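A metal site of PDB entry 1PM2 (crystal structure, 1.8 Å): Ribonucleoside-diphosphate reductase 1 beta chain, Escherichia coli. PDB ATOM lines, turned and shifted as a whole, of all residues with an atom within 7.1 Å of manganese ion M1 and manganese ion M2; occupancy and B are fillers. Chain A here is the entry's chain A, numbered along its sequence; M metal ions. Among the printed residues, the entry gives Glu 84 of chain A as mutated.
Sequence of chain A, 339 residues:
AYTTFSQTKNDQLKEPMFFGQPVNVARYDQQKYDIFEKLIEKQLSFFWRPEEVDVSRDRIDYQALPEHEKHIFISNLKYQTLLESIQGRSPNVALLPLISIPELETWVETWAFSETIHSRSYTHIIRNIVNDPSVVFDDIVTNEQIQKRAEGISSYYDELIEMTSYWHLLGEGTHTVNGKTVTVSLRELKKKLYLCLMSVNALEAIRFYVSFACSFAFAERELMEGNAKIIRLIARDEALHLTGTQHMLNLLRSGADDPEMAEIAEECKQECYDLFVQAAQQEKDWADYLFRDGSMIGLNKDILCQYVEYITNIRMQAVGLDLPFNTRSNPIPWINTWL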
ATOM      1  N   GLN A  43     -10.305   0.606  18.828  1.00  0.00           N
ATOM      2  CA  GLN A  43     -11.204   1.415  18.013  1.00  0.00           C
ATOM      3  C   GLN A  43     -10.910   2.905  18.196  1.00  0.00           C
ATOM      4  O   GLN A  43     -10.931   3.670  17.233  1.00  0.00           O
ATOM      5  CB  GLN A  43     -12.670   1.108  18.357  1.00  0.00           C
ATOM      6  CG  GLN A  43     -13.680   1.816  17.463  1.00  0.00           C
ATOM      7  CD  GLN A  43     -13.577   1.416  15.996  1.00  0.00           C
ATOM      8  OE1 GLN A  43     -14.193   0.440  15.560  1.00  0.00           O
ATOM      9  NE2 GLN A  43     -12.798   2.174  15.228  1.00  0.00           N
ATOM     10  N   GLN A  80     -23.885  -0.526   0.979  1.00  0.00           N
ATOM     11  CA  GLN A  80     -22.992  -0.276   2.096  1.00  0.00           C
ATOM     12  C   GLN A  80     -23.617   0.814   2.982  1.00  0.00           C
ATOM     13  O   GLN A  80     -23.588   0.716   4.207  1.00  0.00           O
ATOM     14  CB  GLN A  80     -21.619   0.195   1.588  1.00  0.00           C
ATOM     15  CG  GLN A  80     -20.860  -0.838   0.749  1.00  0.00           C
ATOM     16  CD  GLN A  80     -19.548  -0.315   0.191  1.00  0.00           C
ATOM     17  OE1 GLN A  80     -19.476   0.803  -0.331  1.00  0.00           O
ATOM     18  NE2 GLN A  80     -18.500  -1.126   0.283  1.00  0.00           N
ATOM     19  N   LEU A  83     -26.459  -0.604   5.099  1.00  0.00           N
ATOM     20  CA  LEU A  83     -25.939  -1.352   6.237  1.00  0.00           C
ATOM     21  C   LEU A  83     -25.385  -0.462   7.344  1.00  0.00           C
ATOM     22  O   LEU A  83     -25.574  -0.758   8.521  1.00  0.00           O
ATOM     23  CB  LEU A  83     -24.869  -2.341   5.786  1.00  0.00           C
ATOM     24  CG  LEU A  83     -25.325  -3.529   4.925  1.00  0.00           C
ATOM     25  CD1 LEU A  83     -24.155  -4.485   4.742  1.00  0.00           C
ATOM     26  CD2 LEU A  83     -26.495  -4.243   5.585  1.00  0.00           C
ATOM     27  N   GLU A  84     -24.706   0.607   6.980  1.00  0.00           N
ATOM     28  CA  GLU A  84     -24.144   1.517   7.977  1.00  0.00           C
ATOM     29  C   GLU A  84     -25.251   2.296   8.699  1.00  0.00           C
ATOM     30  O   GLU A  84     -25.151   2.590   9.886  1.00  0.00           O
ATOM     31  CB  GLU A  84     -23.138   2.478   7.342  1.00  0.00           C
ATOM     32  CG  GLU A  84     -21.952   1.774   6.690  1.00  0.00           C
ATOM     33  CD  GLU A  84     -21.009   1.125   7.696  1.00  0.00           C
ATOM     34  OE1 GLU A  84     -21.378   1.006   8.881  1.00  0.00           O
ATOM     35  OE2 GLU A  84     -19.898   0.733   7.286  1.00  0.00           O
ATOM     36  N   GLN A  87     -26.507  -0.185  11.143  1.00  0.00           N
ATOM     37  CA  GLN A  87     -25.502  -0.474  12.165  1.00  0.00           C
ATOM     38  C   GLN A  87     -25.144   0.702  13.050  1.00  0.00           C
ATOM     39  O   GLN A  87     -24.566   0.520  14.121  1.00  0.00           O
ATOM     40  CB  GLN A  87     -24.241  -1.051  11.519  1.00  0.00           C
ATOM     41  CG  GLN A  87     -24.390  -2.497  11.057  1.00  0.00           C
ATOM     42  CD  GLN A  87     -24.948  -3.395  12.149  1.00  0.00           C
ATOM     43  OE1 GLN A  87     -26.167  -3.482  12.342  1.00  0.00           O
ATOM     44  NE2 GLN A  87     -24.062  -4.039  12.892  1.00  0.00           N
ATOM     45  N   TRP A 111     -18.685   0.938  19.189  1.00  0.00           N
ATOM     46  CA  TRP A 111     -18.859   0.222  17.936  1.00  0.00           C
ATOM     47  C   TRP A 111     -19.924   0.952  17.117  1.00  0.00           C
ATOM     48  O   TRP A 111     -19.714   1.270  15.937  1.00  0.00           O
ATOM     49  CB  TRP A 111     -19.263  -1.221  18.279  1.00  0.00           C
ATOM     50  CG  TRP A 111     -19.911  -2.048  17.209  1.00  0.00           C
ATOM     51  CD1 TRP A 111     -19.855  -1.868  15.850  1.00  0.00           C
ATOM     52  CD2 TRP A 111     -20.666  -3.247  17.419  1.00  0.00           C
ATOM     53  NE1 TRP A 111     -20.535  -2.875  15.213  1.00  0.00           N
ATOM     54  CE2 TRP A 111     -21.042  -3.739  16.159  1.00  0.00           C
ATOM     55  CE3 TRP A 111     -21.063  -3.946  18.571  1.00  0.00           C
ATOM     56  CZ2 TRP A 111     -21.805  -4.911  16.001  1.00  0.00           C
ATOM     57  CZ3 TRP A 111     -21.816  -5.110  18.416  1.00  0.00           C
ATOM     58  CH2 TRP A 111     -22.176  -5.578  17.133  1.00  0.00           C
ATOM     59  N   SER A 114     -18.653   4.272  15.747  1.00  0.00           N
ATOM     60  CA  SER A 114     -17.784   4.113  14.581  1.00  0.00           C
ATOM     61  C   SER A 114     -18.598   3.874  13.310  1.00  0.00           C
ATOM     62  O   SER A 114     -18.183   4.261  12.218  1.00  0.00           O
ATOM     63  CB  SER A 114     -16.777   2.985  14.792  1.00  0.00           C
ATOM     64  OG  SER A 114     -17.401   1.709  14.767  1.00  0.00           O
ATOM     65  N   GLU A 115     -19.769   3.239  13.440  1.00  0.00           N
ATOM     66  CA  GLU A 115     -20.609   2.981  12.283  1.00  0.00           C
ATOM     67  C   GLU A 115     -21.206   4.301  11.775  1.00  0.00           C
ATOM     68  O   GLU A 115     -21.394   4.471  10.568  1.00  0.00           O
ATOM     69  CB  GLU A 115     -21.730   1.990  12.631  1.00  0.00           C
ATOM     70  CG  GLU A 115     -21.235   0.674  13.235  1.00  0.00           C
ATOM     71  CD  GLU A 115     -20.606  -0.259  12.209  1.00  0.00           C
ATOM     72  OE1 GLU A 115     -19.893   0.214  11.305  1.00  0.00           O
ATOM     73  OE2 GLU A 115     -20.817  -1.490  12.335  1.00  0.00           O
ATOM     74  N   THR A 116     -21.504   5.237  12.674  1.00  0.00           N
ATOM     75  CA  THR A 116     -22.068   6.513  12.228  1.00  0.00           C
ATOM     76  C   THR A 116     -20.989   7.276  11.474  1.00  0.00           C
ATOM     77  O   THR A 116     -21.292   8.069  10.575  1.00  0.00           O
ATOM     78  CB  THR A 116     -22.575   7.400  13.393  1.00  0.00           C
ATOM     79  OG1 THR A 116     -21.478   7.829  14.210  1.00  0.00           O
ATOM     80  CG2 THR A 116     -23.584   6.644  14.234  1.00  0.00           C
ATOM     81  N   ILE A 117     -19.728   7.050  11.831  1.00  0.00           N
ATOM     82  CA  ILE A 117     -18.630   7.709  11.127  1.00  0.00           C
ATOM     83  C   ILE A 117     -18.579   7.125   9.720  1.00  0.00           C
ATOM     84  O   ILE A 117     -18.348   7.836   8.743  1.00  0.00           O
ATOM     85  CB  ILE A 117     -17.273   7.477  11.835  1.00  0.00           C
ATOM     86  CG1 ILE A 117     -17.261   8.203  13.188  1.00  0.00           C
ATOM     87  CG2 ILE A 117     -16.123   7.983  10.960  1.00  0.00           C
ATOM     88  CD1 ILE A 117     -17.387   9.720  13.087  1.00  0.00           C
ATOM     89  N   HIS A 118     -18.808   5.816   9.630  1.00  0.00           N
ATOM     90  CA  HIS A 118     -18.820   5.157   8.320  1.00  0.00           C
ATOM     91  C   HIS A 118     -19.934   5.757   7.474  1.00  0.00           C
ATOM     92  O   HIS A 118     -19.748   6.028   6.281  1.00  0.00           O
ATOM     93  CB  HIS A 118     -19.026   3.647   8.494  1.00  0.00           C
ATOM     94  CG  HIS A 118     -17.901   2.960   9.208  1.00  0.00           C
ATOM     95  ND1 HIS A 118     -17.917   1.616   9.487  1.00  0.00           N
ATOM     96  CD2 HIS A 118     -16.730   3.436   9.701  1.00  0.00           C
ATOM     97  CE1 HIS A 118     -16.813   1.289  10.125  1.00  0.00           C
ATOM     98  NE2 HIS A 118     -16.074   2.378  10.270  1.00  0.00           N
ATOM     99  N   SER A 119     -21.097   5.974   8.084  1.00  0.00           N
ATOM    100  CA  SER A 119     -22.234   6.567   7.371  1.00  0.00           C
ATOM    101  C   SER A 119     -21.833   7.962   6.876  1.00  0.00           C
ATOM    102  O   SER A 119     -22.152   8.349   5.754  1.00  0.00           O
ATOM    103  CB  SER A 119     -23.454   6.698   8.287  1.00  0.00           C
ATOM    104  OG  SER A 119     -23.980   5.423   8.619  1.00  0.00           O
ATOM    105  N   TYR A 122     -19.757   7.866   3.774  1.00  0.00           N
ATOM    106  CA  TYR A 122     -20.482   7.593   2.535  1.00  0.00           C
ATOM    107  C   TYR A 122     -21.185   8.842   2.015  1.00  0.00           C
ATOM    108  O   TYR A 122     -21.323   9.020   0.803  1.00  0.00           O
ATOM    109  CB  TYR A 122     -21.464   6.435   2.734  1.00  0.00           C
ATOM    110  CG  TYR A 122     -20.763   5.094   2.735  1.00  0.00           C
ATOM    111  CD1 TYR A 122     -19.971   4.713   1.658  1.00  0.00           C
ATOM    112  CD2 TYR A 122     -20.861   4.223   3.822  1.00  0.00           C
ATOM    113  CE1 TYR A 122     -19.290   3.499   1.649  1.00  0.00           C
ATOM    114  CE2 TYR A 122     -20.177   2.998   3.829  1.00  0.00           C
ATOM    115  CZ  TYR A 122     -19.398   2.641   2.736  1.00  0.00           C
ATOM    116  OH  TYR A 122     -18.716   1.450   2.729  1.00  0.00           O
ATOM    117  N   LEU A 203     -23.422 -10.178   9.180  1.00  0.00           N
ATOM    118  CA  LEU A 203     -23.506  -8.866   8.537  1.00  0.00           C
ATOM    119  C   LEU A 203     -22.107  -8.224   8.511  1.00  0.00           C
ATOM    120  O   LEU A 203     -21.621  -7.817   7.465  1.00  0.00           O
ATOM    121  CB  LEU A 203     -24.488  -7.971   9.309  1.00  0.00           C
ATOM    122  CG  LEU A 203     -24.849  -6.584   8.748  1.00  0.00           C
ATOM    123  CD1 LEU A 203     -26.041  -6.041   9.527  1.00  0.00           C
ATOM    124  CD2 LEU A 203     -23.671  -5.621   8.854  1.00  0.00           C
ATOM    125  N   GLU A 204     -21.483  -8.179   9.683  1.00  0.00           N
ATOM    126  CA  GLU A 204     -20.148  -7.578   9.836  1.00  0.00           C
ATOM    127  C   GLU A 204     -19.030  -8.335   9.114  1.00  0.00           C
ATOM    128  O   GLU A 204     -18.191  -7.733   8.450  1.00  0.00           O
ATOM    129  CB  GLU A 204     -19.791  -7.514  11.330  1.00  0.00           C
ATOM    130  CG  GLU A 204     -20.726  -6.705  12.229  1.00  0.00           C
ATOM    131  CD  GLU A 204     -20.477  -5.206  12.160  1.00  0.00           C
ATOM    132  OE1 GLU A 204     -19.404  -4.803  11.645  1.00  0.00           O
ATOM    133  OE2 GLU A 204     -21.333  -4.425  12.626  1.00  0.00           O
ATOM    134  N   PHE A 208     -20.404  -7.067   4.665  1.00  0.00           N
ATOM    135  CA  PHE A 208     -19.502  -5.925   4.473  1.00  0.00           C
ATOM    136  C   PHE A 208     -18.301  -6.282   3.583  1.00  0.00           C
ATOM    137  O   PHE A 208     -17.935  -5.510   2.703  1.00  0.00           O
ATOM    138  CB  PHE A 208     -18.975  -5.389   5.815  1.00  0.00           C
ATOM    139  CG  PHE A 208     -19.878  -4.373   6.467  1.00  0.00           C
ATOM    140  CD1 PHE A 208     -20.431  -3.337   5.717  1.00  0.00           C
ATOM    141  CD2 PHE A 208     -20.147  -4.436   7.825  1.00  0.00           C
ATOM    142  CE1 PHE A 208     -21.241  -2.370   6.330  1.00  0.00           C
ATOM    143  CE2 PHE A 208     -20.955  -3.475   8.446  1.00  0.00           C
ATOM    144  CZ  PHE A 208     -21.500  -2.434   7.685  1.00  0.00           C
ATOM    145  N   PHE A 212     -16.687  -4.874   0.101  1.00  0.00           N
ATOM    146  CA  PHE A 212     -15.345  -4.313   0.009  1.00  0.00           C
ATOM    147  C   PHE A 212     -14.681  -4.800  -1.267  1.00  0.00           C
ATOM    148  O   PHE A 212     -13.995  -4.032  -1.949  1.00  0.00           O
ATOM    149  CB  PHE A 212     -14.487  -4.717   1.216  1.00  0.00           C
ATOM    150  CG  PHE A 212     -14.987  -4.215   2.541  1.00  0.00           C
ATOM    151  CD1 PHE A 212     -15.797  -3.097   2.623  1.00  0.00           C
ATOM    152  CD2 PHE A 212     -14.630  -4.871   3.723  1.00  0.00           C
ATOM    153  CE1 PHE A 212     -16.258  -2.623   3.849  1.00  0.00           C
ATOM    154  CE2 PHE A 212     -15.080  -4.410   4.950  1.00  0.00           C
ATOM    155  CZ  PHE A 212     -15.892  -3.287   5.024  1.00  0.00           C
ATOM    156  N   ILE A 234     -12.657   1.865   6.779  1.00  0.00           N
ATOM    157  CA  ILE A 234     -13.868   1.203   7.250  1.00  0.00           C
ATOM    158  C   ILE A 234     -13.586  -0.268   7.544  1.00  0.00           C
ATOM    159  O   ILE A 234     -13.983  -0.794   8.590  1.00  0.00           O
ATOM    160  CB  ILE A 234     -15.006   1.293   6.199  1.00  0.00           C
ATOM    161  CG1 ILE A 234     -15.490   2.743   6.103  1.00  0.00           C
ATOM    162  CG2 ILE A 234     -16.156   0.361   6.592  1.00  0.00           C
ATOM    163  CD1 ILE A 234     -16.609   2.956   5.080  1.00  0.00           C
ATOM    164  N   ALA A 235     -12.899  -0.943   6.624  1.00  0.00           N
ATOM    165  CA  ALA A 235     -12.573  -2.353   6.790  1.00  0.00           C
ATOM    166  C   ALA A 235     -11.739  -2.587   8.053  1.00  0.00           C
ATOM    167  O   ALA A 235     -11.899  -3.595   8.725  1.00  0.00           O
ATOM    168  CB  ALA A 235     -11.816  -2.871   5.560  1.00  0.00           C
ATOM    169  N   ASP A 237     -11.982  -0.978  10.747  1.00  0.00           N
ATOM    170  CA  ASP A 237     -12.927  -0.899  11.851  1.00  0.00           C
ATOM    171  C   ASP A 237     -13.799  -2.151  11.906  1.00  0.00           C
ATOM    172  O   ASP A 237     -14.029  -2.713  12.967  1.00  0.00           O
ATOM    173  CB  ASP A 237     -13.845   0.325  11.710  1.00  0.00           C
ATOM    174  CG  ASP A 237     -13.114   1.640  11.895  1.00  0.00           C
ATOM    175  OD1 ASP A 237     -12.074   1.662  12.579  1.00  0.00           O
ATOM    176  OD2 ASP A 237     -13.609   2.661  11.365  1.00  0.00           O
ATOM    177  N   GLU A 238     -14.286  -2.589  10.741  1.00  0.00           N
ATOM    178  CA  GLU A 238     -15.122  -3.772  10.676  1.00  0.00           C
ATOM    179  C   GLU A 238     -14.410  -4.997  11.233  1.00  0.00           C
ATOM    180  O   GLU A 238     -15.047  -5.879  11.820  1.00  0.00           O
ATOM    181  CB  GLU A 238     -15.575  -4.039   9.227  1.00  0.00           C
ATOM    182  CG  GLU A 238     -16.307  -2.876   8.584  1.00  0.00           C
ATOM    183  CD  GLU A 238     -17.541  -2.435   9.366  1.00  0.00           C
ATOM    184  OE1 GLU A 238     -18.121  -1.387   9.005  1.00  0.00           O
ATOM    185  OE2 GLU A 238     -17.952  -3.136  10.314  1.00  0.00           O
ATOM    186  N   ALA A 239     -13.087  -5.048  11.062  1.00  0.00           N
ATOM    187  CA  ALA A 239     -12.311  -6.173  11.576  1.00  0.00           C
ATOM    188  C   ALA A 239     -12.463  -6.247  13.095  1.00  0.00           C
ATOM    189  O   ALA A 239     -12.562  -7.339  13.677  1.00  0.00           O
ATOM    190  CB  ALA A 239     -10.841  -6.008  11.212  1.00  0.00           C
ATOM    191  N   LEU A 240     -12.474  -5.091  13.741  1.00  0.00           N
ATOM    192  CA  LEU A 240     -12.639  -5.037  15.189  1.00  0.00           C
ATOM    193  C   LEU A 240     -14.047  -5.449  15.573  1.00  0.00           C
ATOM    194  O   LEU A 240     -14.256  -6.158  16.559  1.00  0.00           O
ATOM    195  CB  LEU A 240     -12.393  -3.615  15.724  1.00  0.00           C
ATOM    196  CG  LEU A 240     -11.002  -3.009  15.567  1.00  0.00           C
ATOM    197  CD1 LEU A 240     -11.013  -1.599  16.147  1.00  0.00           C
ATOM    198  CD2 LEU A 240      -9.974  -3.880  16.279  1.00  0.00           C
ATOM    199  N   HIS A 241     -15.024  -4.980  14.808  1.00  0.00           N
ATOM    200  CA  HIS A 241     -16.417  -5.281  15.067  1.00  0.00           C
ATOM    201  C   HIS A 241     -16.712  -6.771  15.018  1.00  0.00           C
ATOM    202  O   HIS A 241     -17.356  -7.323  15.917  1.00  0.00           O
ATOM    203  CB  HIS A 241     -17.316  -4.549  14.069  1.00  0.00           C
ATOM    204  CG  HIS A 241     -17.138  -3.061  14.093  1.00  0.00           C
ATOM    205  ND1 HIS A 241     -17.740  -2.228  13.184  1.00  0.00           N
ATOM    206  CD2 HIS A 241     -16.430  -2.263  14.927  1.00  0.00           C
ATOM    207  CE1 HIS A 241     -17.412  -0.973  13.450  1.00  0.00           C
ATOM    208  NE2 HIS A 241     -16.611  -0.972  14.496  1.00  0.00           N
ATOM    209  N   LEU A 242     -16.224  -7.449  13.981  1.00  0.00           N
ATOM    210  CA  LEU A 242     -16.481  -8.880  13.866  1.00  0.00           C
ATOM    211  C   LEU A 242     -15.692  -9.645  14.925  1.00  0.00           C
ATOM    212  O   LEU A 242     -16.101 -10.714  15.355  1.00  0.00           O
ATOM    213  CB  LEU A 242     -16.164  -9.371  12.452  1.00  0.00           C
ATOM    214  CG  LEU A 242     -14.731  -9.415  11.936  1.00  0.00           C
ATOM    215  CD1 LEU A 242     -14.074 -10.709  12.388  1.00  0.00           C
ATOM    216  CD2 LEU A 242     -14.734  -9.324  10.410  1.00  0.00           C
HETATM  217 MN    MN M   1     -19.167  -2.710  11.845  1.00  0.00          MN
HETATM  218 MN    MN M   2     -19.293   0.123   9.271  1.00  0.00          MN
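A ring nitrogen (NE2) of His 241 is in hydrogen-bond range of the side-chain hydroxyl of Ser 114.
NE2 of His 118 sits close to O of Ser 114.
NE1 of Trp 111 sits close to OE2 of Glu 115, 3.2 Å away.
The backbone carbonyl oxygen of Glu 115 sits at hydrogen-bond distance from the side-chain hydroxyl of Ser 119.
OE2 of Glu 204 sits at hydrogen-bond distance from NE1 of Trp 111 (3.1 Å).
The side-chain hydroxyl of Ser 119 sits at hydrogen-bond distance from the backbone carbonyl oxygen of Glu 84 (3.3 Å).
The backbone carbonyl oxygen (O) of Trp 111 lies within hydrogen-bond range of the side-chain hydroxyl (OG) of Ser 114 (2.6 Å).
O of Leu 203 sits at hydrogen-bond distance from N of Phe 208 (3.1 Å).
Manganese ion M1 is bound by OE2 of Glu 238 (2.0 Å), ND1 of His 241 (2.0 Å), OE2 of Glu 115 (2.1 Å) and OE1 of Glu 204 (2.1 Å).
Manganese ion M1 has four donor atoms within binding distance.
Slightly farther from manganese ion M1 lies the side-chain carboxylate (OE2) of Glu 204 (2.9 Å).
Manganese ion M2 is bound by OE1 of Glu 238, ND1 of His 118, OE1 of Glu 115, OE2 of Glu 84 and OE1 of Glu 84.
Trp 111 touches manganese ion M1 (NE1 to MN, 3.6 Å).
CE2 of Phe 208 touches manganese ion M1, at 3.9 Å.
Within 4 Å of manganese ion M1: Trp 111, Glu 115, Glu 204, Phe 208, Glu 238 and His 241.
Merely in contact with manganese ion M2: Phe 208 (3.7 Å).
Five residues have an atom within 4 Å of manganese ion M2: Glu 84, Glu 115, His 118, Phe 208 and Glu 238.
The nearest printed residue that does not touch manganese ion M2 is Ile 234 (4.1 Å).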
